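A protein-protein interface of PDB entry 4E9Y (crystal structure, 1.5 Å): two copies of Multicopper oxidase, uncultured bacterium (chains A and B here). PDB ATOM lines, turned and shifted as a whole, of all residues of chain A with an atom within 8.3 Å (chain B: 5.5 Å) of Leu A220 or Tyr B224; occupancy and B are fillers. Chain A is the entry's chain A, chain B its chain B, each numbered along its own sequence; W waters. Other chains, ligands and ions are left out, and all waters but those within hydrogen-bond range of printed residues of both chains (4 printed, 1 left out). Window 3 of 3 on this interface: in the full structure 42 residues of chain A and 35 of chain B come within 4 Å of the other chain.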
ATOM      1  N   LEU A 130      -4.065  35.027 -13.023  1.00  0.00           N
ATOM      2  CA  LEU A 130      -3.198  34.909 -11.860  1.00  0.00           C
ATOM      3  C   LEU A 130      -3.147  36.256 -11.162  1.00  0.00           C
ATOM      4  O   LEU A 130      -3.237  37.259 -11.866  1.00  0.00           O
ATOM      5  CB  LEU A 130      -1.758  34.534 -12.225  1.00  0.00           C
ATOM      6  CG  LEU A 130      -1.534  33.240 -13.006  1.00  0.00           C
ATOM      7  CD1 LEU A 130      -0.075  33.068 -13.399  1.00  0.00           C
ATOM      8  CD2 LEU A 130      -1.989  32.040 -12.186  1.00  0.00           C
ATOM      9  N   LEU A 211      10.224  35.952 -15.296  1.00  0.00           N
ATOM     10  CA  LEU A 211       9.538  34.931 -14.528  1.00  0.00           C
ATOM     11  C   LEU A 211       8.613  34.224 -15.522  1.00  0.00           C
ATOM     12  O   LEU A 211       7.682  34.819 -16.052  1.00  0.00           O
ATOM     13  CB  LEU A 211       8.733  35.530 -13.386  1.00  0.00           C
ATOM     14  CG  LEU A 211       7.893  34.502 -12.620  1.00  0.00           C
ATOM     15  CD1 LEU A 211       8.832  33.513 -11.936  1.00  0.00           C
ATOM     16  CD2 LEU A 211       6.971  35.221 -11.645  1.00  0.00           C
ATOM     17  N   VAL A 212       8.931  32.950 -15.787  1.00  0.00           N
ATOM     18  CA  VAL A 212       8.133  32.166 -16.743  1.00  0.00           C
ATOM     19  C   VAL A 212       6.894  31.667 -16.020  1.00  0.00           C
ATOM     20  O   VAL A 212       6.972  30.852 -15.095  1.00  0.00           O
ATOM     21  CB  VAL A 212       8.947  30.996 -17.316  1.00  0.00           C
ATOM     22  CG1 VAL A 212       8.040  30.252 -18.319  1.00  0.00           C
ATOM     23  CG2 VAL A 212      10.240  31.455 -17.973  1.00  0.00           C
ATOM     24  N   THR A 213       5.727  32.181 -16.432  1.00  0.00           N
ATOM     25  CA  THR A 213       4.505  31.845 -15.737  1.00  0.00           C
ATOM     26  C   THR A 213       3.536  30.944 -16.480  1.00  0.00           C
ATOM     27  O   THR A 213       2.655  30.355 -15.828  1.00  0.00           O
ATOM     28  CB  THR A 213       3.736  33.165 -15.434  1.00  0.00           C
ATOM     29  OG1 THR A 213       3.429  33.772 -16.698  1.00  0.00           O
ATOM     30  CG2 THR A 213       4.572  34.146 -14.626  1.00  0.00           C
ATOM     31  N   HIS A 214       3.644  30.864 -17.804  1.00  0.00           N
ATOM     32  CA  HIS A 214       2.686  30.055 -18.567  1.00  0.00           C
ATOM     33  C   HIS A 214       3.381  29.328 -19.717  1.00  0.00           C
ATOM     34  O   HIS A 214       4.234  29.881 -20.393  1.00  0.00           O
ATOM     35  CB  HIS A 214       1.553  30.839 -19.231  1.00  0.00           C
ATOM     36  CG  HIS A 214       0.643  31.628 -18.349  1.00  0.00           C
ATOM     37  ND1 HIS A 214       1.070  32.708 -17.607  1.00  0.00           N
ATOM     38  CD2 HIS A 214      -0.691  31.507 -18.088  1.00  0.00           C
ATOM     39  CE1 HIS A 214       0.062  33.216 -16.927  1.00  0.00           C
ATOM     40  NE2 HIS A 214      -1.028  32.502 -17.211  1.00  0.00           N
ATOM     41  N   LYS A 215       2.967  28.091 -19.909  1.00  0.00           N
ATOM     42  CA  LYS A 215       3.410  27.278 -21.033  1.00  0.00           C
ATOM     43  C   LYS A 215       2.185  26.969 -21.915  1.00  0.00           C
ATOM     44  O   LYS A 215       1.202  26.470 -21.371  1.00  0.00           O
ATOM     45  CB  LYS A 215       4.116  26.037 -20.488  1.00  0.00           C
ATOM     46  CG  LYS A 215       4.155  24.869 -21.439  1.00  0.00           C
ATOM     47  CD  LYS A 215       4.984  25.087 -22.698  1.00  0.00           C
ATOM     48  CE  LYS A 215       4.924  23.807 -23.541  1.00  0.00           C
ATOM     49  NZ  LYS A 215       5.248  24.052 -24.967  1.00  0.00           N
ATOM     50  N   ASP A 216       2.285  27.316 -23.192  1.00  0.00           N
ATOM     51  CA  ASP A 216       1.185  27.161 -24.148  1.00  0.00           C
ATOM     52  C   ASP A 216      -0.114  27.750 -23.638  1.00  0.00           C
ATOM     53  O   ASP A 216      -1.219  27.230 -23.876  1.00  0.00           O
ATOM     54  CB  ASP A 216       0.992  25.667 -24.469  1.00  0.00           C
ATOM     55  CG  ASP A 216       2.251  25.120 -25.159  1.00  0.00           C
ATOM     56  OD1 ASP A 216       3.144  25.872 -25.605  1.00  0.00           O
ATOM     57  OD2 ASP A 216       2.327  23.878 -25.223  1.00  0.00           O
ATOM     58  N   GLY A 217       0.001  28.873 -22.915  1.00  0.00           N
ATOM     59  CA  GLY A 217      -1.150  29.614 -22.419  1.00  0.00           C
ATOM     60  C   GLY A 217      -1.677  29.160 -21.088  1.00  0.00           C
ATOM     61  O   GLY A 217      -2.536  29.817 -20.488  1.00  0.00           O
ATOM     62  N   LEU A 218      -1.213  28.025 -20.538  1.00  0.00           N
ATOM     63  CA  LEU A 218      -1.767  27.554 -19.270  1.00  0.00           C
ATOM     64  C   LEU A 218      -0.789  27.827 -18.132  1.00  0.00           C
ATOM     65  O   LEU A 218       0.421  27.661 -18.334  1.00  0.00           O
ATOM     66  CB  LEU A 218      -2.061  26.058 -19.374  1.00  0.00           C
ATOM     67  CG  LEU A 218      -3.316  25.737 -20.209  1.00  0.00           C
ATOM     68  CD1 LEU A 218      -3.455  24.232 -20.396  1.00  0.00           C
ATOM     69  CD2 LEU A 218      -4.541  26.351 -19.545  1.00  0.00           C
ATOM     70  N   PRO A 219      -1.261  28.275 -16.976  1.00  0.00           N
ATOM     71  CA  PRO A 219      -0.373  28.740 -15.904  1.00  0.00           C
ATOM     72  C   PRO A 219       0.383  27.590 -15.240  1.00  0.00           C
ATOM     73  O   PRO A 219      -0.220  26.569 -14.874  1.00  0.00           O
ATOM     74  CB  PRO A 219      -1.328  29.363 -14.887  1.00  0.00           C
ATOM     75  CG  PRO A 219      -2.662  28.723 -15.141  1.00  0.00           C
ATOM     76  CD  PRO A 219      -2.693  28.395 -16.605  1.00  0.00           C
ATOM     77  N   LEU A 220       1.691  27.791 -15.080  1.00  0.00           N
ATOM     78  CA  LEU A 220       2.483  26.761 -14.406  1.00  0.00           C
ATOM     79  C   LEU A 220       2.262  26.743 -12.905  1.00  0.00           C
ATOM     80  O   LEU A 220       2.171  27.792 -12.269  1.00  0.00           O
ATOM     81  CB  LEU A 220       3.975  27.019 -14.649  1.00  0.00           C
ATOM     82  CG  LEU A 220       4.455  26.898 -16.100  1.00  0.00           C
ATOM     83  CD1 LEU A 220       5.871  27.433 -16.210  1.00  0.00           C
ATOM     84  CD2 LEU A 220       4.417  25.445 -16.561  1.00  0.00           C
ATOM     85  N   ASP A 221       2.168  25.550 -12.315  1.00  0.00           N
ATOM     86  CA  ASP A 221       2.072  25.459 -10.855  1.00  0.00           C
ATOM     87  C   ASP A 221       3.422  25.891 -10.260  1.00  0.00           C
ATOM     88  O   ASP A 221       3.421  26.414  -9.133  1.00  0.00           O
ATOM     89  CB  ASP A 221       1.763  24.050 -10.378  1.00  0.00           C
ATOM     90  CG  ASP A 221       0.358  23.582 -10.710  1.00  0.00           C
ATOM     91  OD1 ASP A 221      -0.548  24.432 -10.878  1.00  0.00           O
ATOM     92  OD2 ASP A 221       0.153  22.351 -10.796  1.00  0.00           O
ATOM     93  N   SER A 222       4.493  25.642 -10.996  1.00  0.00           N
ATOM     94  CA  SER A 222       5.807  26.040 -10.502  1.00  0.00           C
ATOM     95  C   SER A 222       6.518  26.963 -11.479  1.00  0.00           C
ATOM     96  O   SER A 222       7.369  26.580 -12.277  1.00  0.00           O
ATOM     97  CB  SER A 222       6.663  24.794 -10.257  1.00  0.00           C
ATOM     98  OG  SER A 222       7.833  25.193  -9.578  1.00  0.00           O
ATOM     99  N   PRO A 223       6.170  28.243 -11.432  1.00  0.00           N
ATOM    100  CA  PRO A 223       6.857  29.196 -12.308  1.00  0.00           C
ATOM    101  C   PRO A 223       8.335  29.276 -11.937  1.00  0.00           C
ATOM    102  O   PRO A 223       8.726  28.935 -10.819  1.00  0.00           O
ATOM    103  CB  PRO A 223       6.197  30.530 -11.968  1.00  0.00           C
ATOM    104  CG  PRO A 223       5.603  30.315 -10.603  1.00  0.00           C
ATOM    105  CD  PRO A 223       5.136  28.868 -10.584  1.00  0.00           C
ATOM    106  N   TYR A 224       9.135  29.702 -12.902  1.00  0.00           N
ATOM    107  CA  TYR A 224      10.574  29.731 -12.682  1.00  0.00           C
ATOM    108  C   TYR A 224      11.181  30.905 -13.423  1.00  0.00           C
ATOM    109  O   TYR A 224      10.695  31.294 -14.475  1.00  0.00           O
ATOM    110  CB  TYR A 224      11.270  28.442 -13.136  1.00  0.00           C
ATOM    111  CG  TYR A 224      11.080  28.163 -14.615  1.00  0.00           C
ATOM    112  CD1 TYR A 224      12.036  28.517 -15.555  1.00  0.00           C
ATOM    113  CD2 TYR A 224       9.903  27.534 -15.035  1.00  0.00           C
ATOM    114  CE1 TYR A 224      11.857  28.261 -16.905  1.00  0.00           C
ATOM    115  CE2 TYR A 224       9.710  27.269 -16.383  1.00  0.00           C
ATOM    116  CZ  TYR A 224      10.687  27.636 -17.295  1.00  0.00           C
ATOM    117  OH  TYR A 224      10.457  27.356 -18.636  1.00  0.00           O
ATOM    118  N   TYR A 225      12.261  31.411 -12.810  1.00  0.00           N
ATOM    119  CA  TYR A 225      12.995  32.471 -13.481  1.00  0.00           C
ATOM    120  C   TYR A 225      13.969  31.961 -14.529  1.00  0.00           C
ATOM    121  O   TYR A 225      14.544  30.867 -14.430  1.00  0.00           O
ATOM    122  CB  TYR A 225      13.806  33.243 -12.441  1.00  0.00           C
ATOM    123  CG  TYR A 225      12.988  34.118 -11.532  1.00  0.00           C
ATOM    124  CD1 TYR A 225      12.468  35.320 -12.033  1.00  0.00           C
ATOM    125  CD2 TYR A 225      12.758  33.756 -10.219  1.00  0.00           C
ATOM    126  CE1 TYR A 225      11.716  36.133 -11.192  1.00  0.00           C
ATOM    127  CE2 TYR A 225      12.008  34.563  -9.374  1.00  0.00           C
ATOM    128  CZ  TYR A 225      11.497  35.750  -9.884  1.00  0.00           C
ATOM    129  OH  TYR A 225      10.752  36.533  -9.021  1.00  0.00           O
ATOM    130  N   GLU A 235       5.127  26.388 -29.875  1.00  0.00           N
ATOM    131  CA  GLU A 235       5.013  26.676 -28.459  1.00  0.00           C
ATOM    132  C   GLU A 235       4.715  28.144 -28.141  1.00  0.00           C
ATOM    133  O   GLU A 235       5.046  28.997 -28.972  1.00  0.00           O
ATOM    134  CB  GLU A 235       6.374  26.395 -27.796  1.00  0.00           C
ATOM    135  CG  GLU A 235       6.878  24.935 -27.904  1.00  0.00           C
ATOM    136  CD  GLU A 235       8.025  24.792 -26.894  1.00  0.00           C
ATOM    137  OE1 GLU A 235       9.124  25.213 -27.325  1.00  0.00           O
ATOM    138  OE2 GLU A 235       7.840  24.377 -25.751  1.00  0.00           O
ATOM    139  N   ARG A 236       4.149  28.394 -26.972  1.00  0.00           N
ATOM    140  CA  ARG A 236       4.138  29.761 -26.425  1.00  0.00           C
ATOM    141  C   ARG A 236       4.665  29.709 -24.996  1.00  0.00           C
ATOM    142  O   ARG A 236       4.436  28.734 -24.253  1.00  0.00           O
ATOM    143  CB  ARG A 236       2.730  30.362 -26.444  1.00  0.00           C
ATOM    144  CG  ARG A 236       2.267  30.759 -27.840  1.00  0.00           C
ATOM    145  CD  ARG A 236       1.616  29.602 -28.622  1.00  0.00           C
ATOM    146  NE  ARG A 236       0.431  29.102 -27.937  1.00  0.00           N
ATOM    147  CZ  ARG A 236       0.066  27.827 -27.773  1.00  0.00           C
ATOM    148  NH1 ARG A 236       0.810  26.832 -28.267  1.00  0.00           N
ATOM    149  NH2 ARG A 236      -1.055  27.574 -27.095  1.00  0.00           N
ATOM    150  N   TYR A 237       5.357  30.778 -24.617  1.00  0.00           N
ATOM    151  CA  TYR A 237       5.714  31.009 -23.231  1.00  0.00           C
ATOM    152  C   TYR A 237       5.254  32.419 -22.825  1.00  0.00           C
ATOM    153  O   TYR A 237       5.524  33.285 -23.670  1.00  0.00           O
ATOM    154  CB  TYR A 237       7.225  30.879 -22.998  1.00  0.00           C
ATOM    155  CG  TYR A 237       7.656  29.420 -23.140  1.00  0.00           C
ATOM    156  CD1 TYR A 237       7.642  28.605 -22.007  1.00  0.00           C
ATOM    157  CD2 TYR A 237       8.031  28.903 -24.372  1.00  0.00           C
ATOM    158  CE1 TYR A 237       8.021  27.272 -22.093  1.00  0.00           C
ATOM    159  CE2 TYR A 237       8.415  27.569 -24.459  1.00  0.00           C
ATOM    160  CZ  TYR A 237       8.401  26.783 -23.328  1.00  0.00           C
ATOM    161  OH  TYR A 237       8.768  25.452 -23.395  1.00  0.00           O
ATOM    162  N   ASP A 238       4.624  32.555 -21.680  1.00  0.00           N
ATOM    163  CA  ASP A 238       4.317  33.875 -21.137  1.00  0.00           C
ATOM    164  C   ASP A 238       5.331  34.135 -20.009  1.00  0.00           C
ATOM    165  O   ASP A 238       5.518  33.248 -19.165  1.00  0.00           O
ATOM    166  CB  ASP A 238       2.932  34.024 -20.549  1.00  0.00           C
ATOM    167  CG  ASP A 238       1.745  33.843 -21.476  1.00  0.00           C
ATOM    168  OD1 ASP A 238       1.912  33.361 -22.616  1.00  0.00           O
ATOM    169  OD2 ASP A 238       0.635  34.172 -21.008  1.00  0.00           O
ATOM    170  N   MET B 210      -2.030  18.065 -23.376  1.00  0.00           N
ATOM    171  CA  MET B 210      -1.316  16.929 -22.797  1.00  0.00           C
ATOM    172  C   MET B 210      -0.863  17.279 -21.385  1.00  0.00           C
ATOM    173  O   MET B 210      -0.432  18.438 -21.195  1.00  0.00           O
ATOM    174  CB  MET B 210      -0.098  16.614 -23.643  1.00  0.00           C
ATOM    175  CG  MET B 210      -0.419  16.081 -25.049  1.00  0.00           C
ATOM    176  SD  MET B 210       1.052  15.965 -26.076  1.00  0.00           S
ATOM    177  CE  MET B 210       1.177  17.677 -26.688  1.00  0.00           C
ATOM    178  N   LEU B 211      -0.970  16.368 -20.453  1.00  0.00           N
ATOM    179  CA  LEU B 211      -0.413  16.610 -19.110  1.00  0.00           C
ATOM    180  C   LEU B 211       0.985  15.977 -19.140  1.00  0.00           C
ATOM    181  O   LEU B 211       1.063  14.744 -19.291  1.00  0.00           O
ATOM    182  CB  LEU B 211      -1.306  16.038 -18.021  1.00  0.00           C
ATOM    183  CG  LEU B 211      -0.757  16.180 -16.598  1.00  0.00           C
ATOM    184  CD1 LEU B 211      -0.657  17.641 -16.173  1.00  0.00           C
ATOM    185  CD2 LEU B 211      -1.625  15.415 -15.600  1.00  0.00           C
ATOM    186  N   VAL B 212       2.063  16.749 -19.066  1.00  0.00           N
ATOM    187  CA  VAL B 212       3.412  16.185 -19.020  1.00  0.00           C
ATOM    188  C   VAL B 212       3.697  15.686 -17.607  1.00  0.00           C
ATOM    189  O   VAL B 212       3.724  16.480 -16.647  1.00  0.00           O
ATOM    190  CB  VAL B 212       4.462  17.244 -19.425  1.00  0.00           C
ATOM    191  CG1 VAL B 212       5.838  16.582 -19.431  1.00  0.00           C
ATOM    192  CG2 VAL B 212       4.116  17.851 -20.781  1.00  0.00           C
ATOM    193  N   THR B 213       3.888  14.357 -17.514  1.00  0.00           N
ATOM    194  CA  THR B 213       3.991  13.737 -16.217  1.00  0.00           C
ATOM    195  C   THR B 213       5.397  13.197 -15.941  1.00  0.00           C
ATOM    196  O   THR B 213       5.721  13.097 -14.742  1.00  0.00           O
ATOM    197  CB  THR B 213       2.984  12.566 -16.063  1.00  0.00           C
ATOM    198  OG1 THR B 213       3.257  11.615 -17.095  1.00  0.00           O
ATOM    199  CG2 THR B 213       1.534  13.034 -16.228  1.00  0.00           C
ATOM    200  N   LEU B 220       7.630  13.826 -12.679  1.00  0.00           N
ATOM    201  CA  LEU B 220       7.808  15.204 -12.227  1.00  0.00           C
ATOM    202  C   LEU B 220       7.048  15.507 -10.960  1.00  0.00           C
ATOM    203  O   LEU B 220       5.876  15.153 -10.807  1.00  0.00           O
ATOM    204  CB  LEU B 220       7.263  16.138 -13.318  1.00  0.00           C
ATOM    205  CG  LEU B 220       8.057  16.077 -14.621  1.00  0.00           C
ATOM    206  CD1 LEU B 220       7.410  16.910 -15.732  1.00  0.00           C
ATOM    207  CD2 LEU B 220       9.482  16.594 -14.420  1.00  0.00           C
ATOM    208  N   SER B 222       6.202  18.466 -10.338  1.00  0.00           N
ATOM    209  CA  SER B 222       5.307  19.510 -10.820  1.00  0.00           C
ATOM    210  C   SER B 222       4.954  19.290 -12.280  1.00  0.00           C
ATOM    211  O   SER B 222       5.502  19.881 -13.213  1.00  0.00           O
ATOM    212  CB  SER B 222       5.965  20.890 -10.680  1.00  0.00           C
ATOM    213  OG  SER B 222       4.995  21.908 -10.860  1.00  0.00           O
ATOM    214  N   PRO B 223       4.019  18.398 -12.543  1.00  0.00           N
ATOM    215  CA  PRO B 223       3.644  18.162 -13.941  1.00  0.00           C
ATOM    216  C   PRO B 223       2.963  19.418 -14.458  1.00  0.00           C
ATOM    217  O   PRO B 223       2.496  20.251 -13.682  1.00  0.00           O
ATOM    218  CB  PRO B 223       2.667  16.995 -13.844  1.00  0.00           C
ATOM    219  CG  PRO B 223       2.110  17.107 -12.455  1.00  0.00           C
ATOM    220  CD  PRO B 223       3.272  17.564 -11.590  1.00  0.00           C
ATOM    221  N   TYR B 224       2.936  19.518 -15.784  1.00  0.00           N
ATOM    222  CA  TYR B 224       2.383  20.731 -16.375  1.00  0.00           C
ATOM    223  C   TYR B 224       1.702  20.380 -17.695  1.00  0.00           C
ATOM    224  O   TYR B 224       2.051  19.434 -18.395  1.00  0.00           O
ATOM    225  CB  TYR B 224       3.491  21.762 -16.625  1.00  0.00           C
ATOM    226  CG  TYR B 224       4.580  21.257 -17.546  1.00  0.00           C
ATOM    227  CD1 TYR B 224       4.586  21.525 -18.914  1.00  0.00           C
ATOM    228  CD2 TYR B 224       5.628  20.477 -17.032  1.00  0.00           C
ATOM    229  CE1 TYR B 224       5.581  21.054 -19.740  1.00  0.00           C
ATOM    230  CE2 TYR B 224       6.631  20.003 -17.859  1.00  0.00           C
ATOM    231  CZ  TYR B 224       6.609  20.295 -19.221  1.00  0.00           C
ATOM    232  OH  TYR B 224       7.593  19.837 -20.080  1.00  0.00           O
ATOM    233  N   TYR B 225       0.713  21.191 -18.055  1.00  0.00           N
ATOM    234  CA  TYR B 225       0.013  21.015 -19.319  1.00  0.00           C
ATOM    235  C   TYR B 225       0.741  21.689 -20.454  1.00  0.00           C
ATOM    236  O   TYR B 225       1.408  22.722 -20.320  1.00  0.00           O
ATOM    237  CB  TYR B 225      -1.389  21.628 -19.225  1.00  0.00           C
ATOM    238  CG  TYR B 225      -2.361  20.816 -18.403  1.00  0.00           C
ATOM    239  CD1 TYR B 225      -2.919  19.641 -18.927  1.00  0.00           C
ATOM    240  CD2 TYR B 225      -2.713  21.224 -17.127  1.00  0.00           C
ATOM    241  CE1 TYR B 225      -3.814  18.894 -18.169  1.00  0.00           C
ATOM    242  CE2 TYR B 225      -3.609  20.477 -16.382  1.00  0.00           C
ATOM    243  CZ  TYR B 225      -4.153  19.315 -16.905  1.00  0.00           C
ATOM    244  OH  TYR B 225      -5.049  18.582 -16.139  1.00  0.00           O
ATOM    245  N   ALA B 226       0.585  21.082 -21.626  1.00  0.00           N
ATOM    246  CA  ALA B 226       1.204  21.585 -22.826  1.00  0.00           C
ATOM    247  C   ALA B 226       0.359  21.156 -24.025  1.00  0.00           C
ATOM    248  O   ALA B 226      -0.254  20.084 -23.965  1.00  0.00           O
ATOM    249  CB  ALA B 226       2.623  21.057 -23.060  1.00  0.00           C
ATOM    250  N   TYR B 237       9.621  12.016 -22.994  1.00  0.00           N
ATOM    251  CA  TYR B 237       8.586  12.688 -22.240  1.00  0.00           C
ATOM    252  C   TYR B 237       7.362  11.766 -22.185  1.00  0.00           C
ATOM    253  O   TYR B 237       7.055  11.201 -23.258  1.00  0.00           O
ATOM    254  CB  TYR B 237       8.166  14.040 -22.862  1.00  0.00           C
ATOM    255  CG  TYR B 237       9.276  15.074 -22.628  1.00  0.00           C
ATOM    256  CD1 TYR B 237       9.227  15.898 -21.508  1.00  0.00           C
ATOM    257  CD2 TYR B 237      10.335  15.212 -23.503  1.00  0.00           C
ATOM    258  CE1 TYR B 237      10.248  16.839 -21.306  1.00  0.00           C
ATOM    259  CE2 TYR B 237      11.373  16.129 -23.340  1.00  0.00           C
ATOM    260  CZ  TYR B 237      11.277  16.931 -22.213  1.00  0.00           C
ATOM    261  OH  TYR B 237      12.311  17.859 -22.009  1.00  0.00           O
HETATM  262  O   HOH W   1       1.772  20.502 -11.000  1.00  0.00           O
HETATM  263  O   HOH W   2       4.599  23.665 -13.128  1.00  0.00           O
HETATM  264  O   HOH W   3       1.995  23.157 -13.986  1.00  0.00           O
HETATM  265  O   HOH W   4       0.403  23.462 -16.283  1.00  0.00           O
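The backbone carbonyl oxygen (O) of Thr A213 is in hydrogen-bond range of the backbone NH (N) of Leu A220, 2.8 Å away.
The side-chain amino group (NZ) of Lys A215 is in salt-bridge range of the side-chain carboxylate (OD1) of Asp A216.
The side-chain amino group (NZ) of Lys A215 is in salt-bridge range of the side-chain carboxylate (OE2) of Glu A235, at 2.7 Å.
OD1 of Asp A216 lies within salt-bridge range of NH1 of Arg A236 (3.7 Å).
The backbone NH (N) of Met B210 lies within hydrogen-bond range of the backbone carbonyl oxygen (O) of Ala B226 (2.8 Å).
N of Val B212 lies within hydrogen-bond range of O of Tyr B224 (2.8 Å).
Among the printed residues, pairs that only touch across the chains: Ser A222 with Ser B222, Asp A216 with Ala B226, Leu A218 with Tyr B225, Lys A215 with Ala B226, Lys A215 with Tyr B225, Leu A220 with Tyr B224 and Asp A221 with Ser B222.
Printed residues of chain B within 4 Å of Lys A215: Tyr B225 and Ala B226.
Of the printed residues of chain B, Asp A216 touches Ala B226.
Of the printed residues of chain B, Leu A218 touches Tyr B225 (3.5 Å).
Of chain B, only Tyr B224 comes within 4 Å of Leu A220.
Of the printed residues of chain B, Asp A221 touches Ser B222.
Of the printed residues of chain B, Ser A222 touches Ser B222 (3.4 Å).
No residue of chain A comes within 4 Å of Val B212.
Tyr B224 touches just one residue of chain A: Leu A220 (3.8 Å).
The nearest residue of chain A that does not touch Tyr B224 is Lys A215 (4.2 Å).
Of the 20 printed residues of chain A, 6 touch a printed residue of chain B.
Of the 11 printed residues of chain B, 4 touch a printed residue of chain A.
Hydrophobic or aromatic side chains of chain B that line the printed part of chain A: Tyr B224, Tyr B225 and Ala B226.
Along chain B the printed residues that touch a printed residue of chain A span positions 222 to 226.
Leu A220 touches Tyr B224, but with the chains exchanged Tyr A224 does not touch Leu B220 (10.6 Å).
Ser B222 touches its own counterpart, Ser A222.
Water W1 bridges OD2 of Asp A221 and O of Pro B223.
Water W2 lies within hydrogen-bond range of OG of Ser B222 (2.9 Å), N of Ser A222 (2.9 Å) and N of Asp A221 (3.2 Å).
Water W4 lies within hydrogen-bond range of the backbone NH of Tyr B225 (2.9 Å) and the backbone carbonyl oxygen of Pro A219 (3.5 Å).
Water W3 bridges N of Asp A221 (2.9 Å) and O of Pro B223 (3.0 Å).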
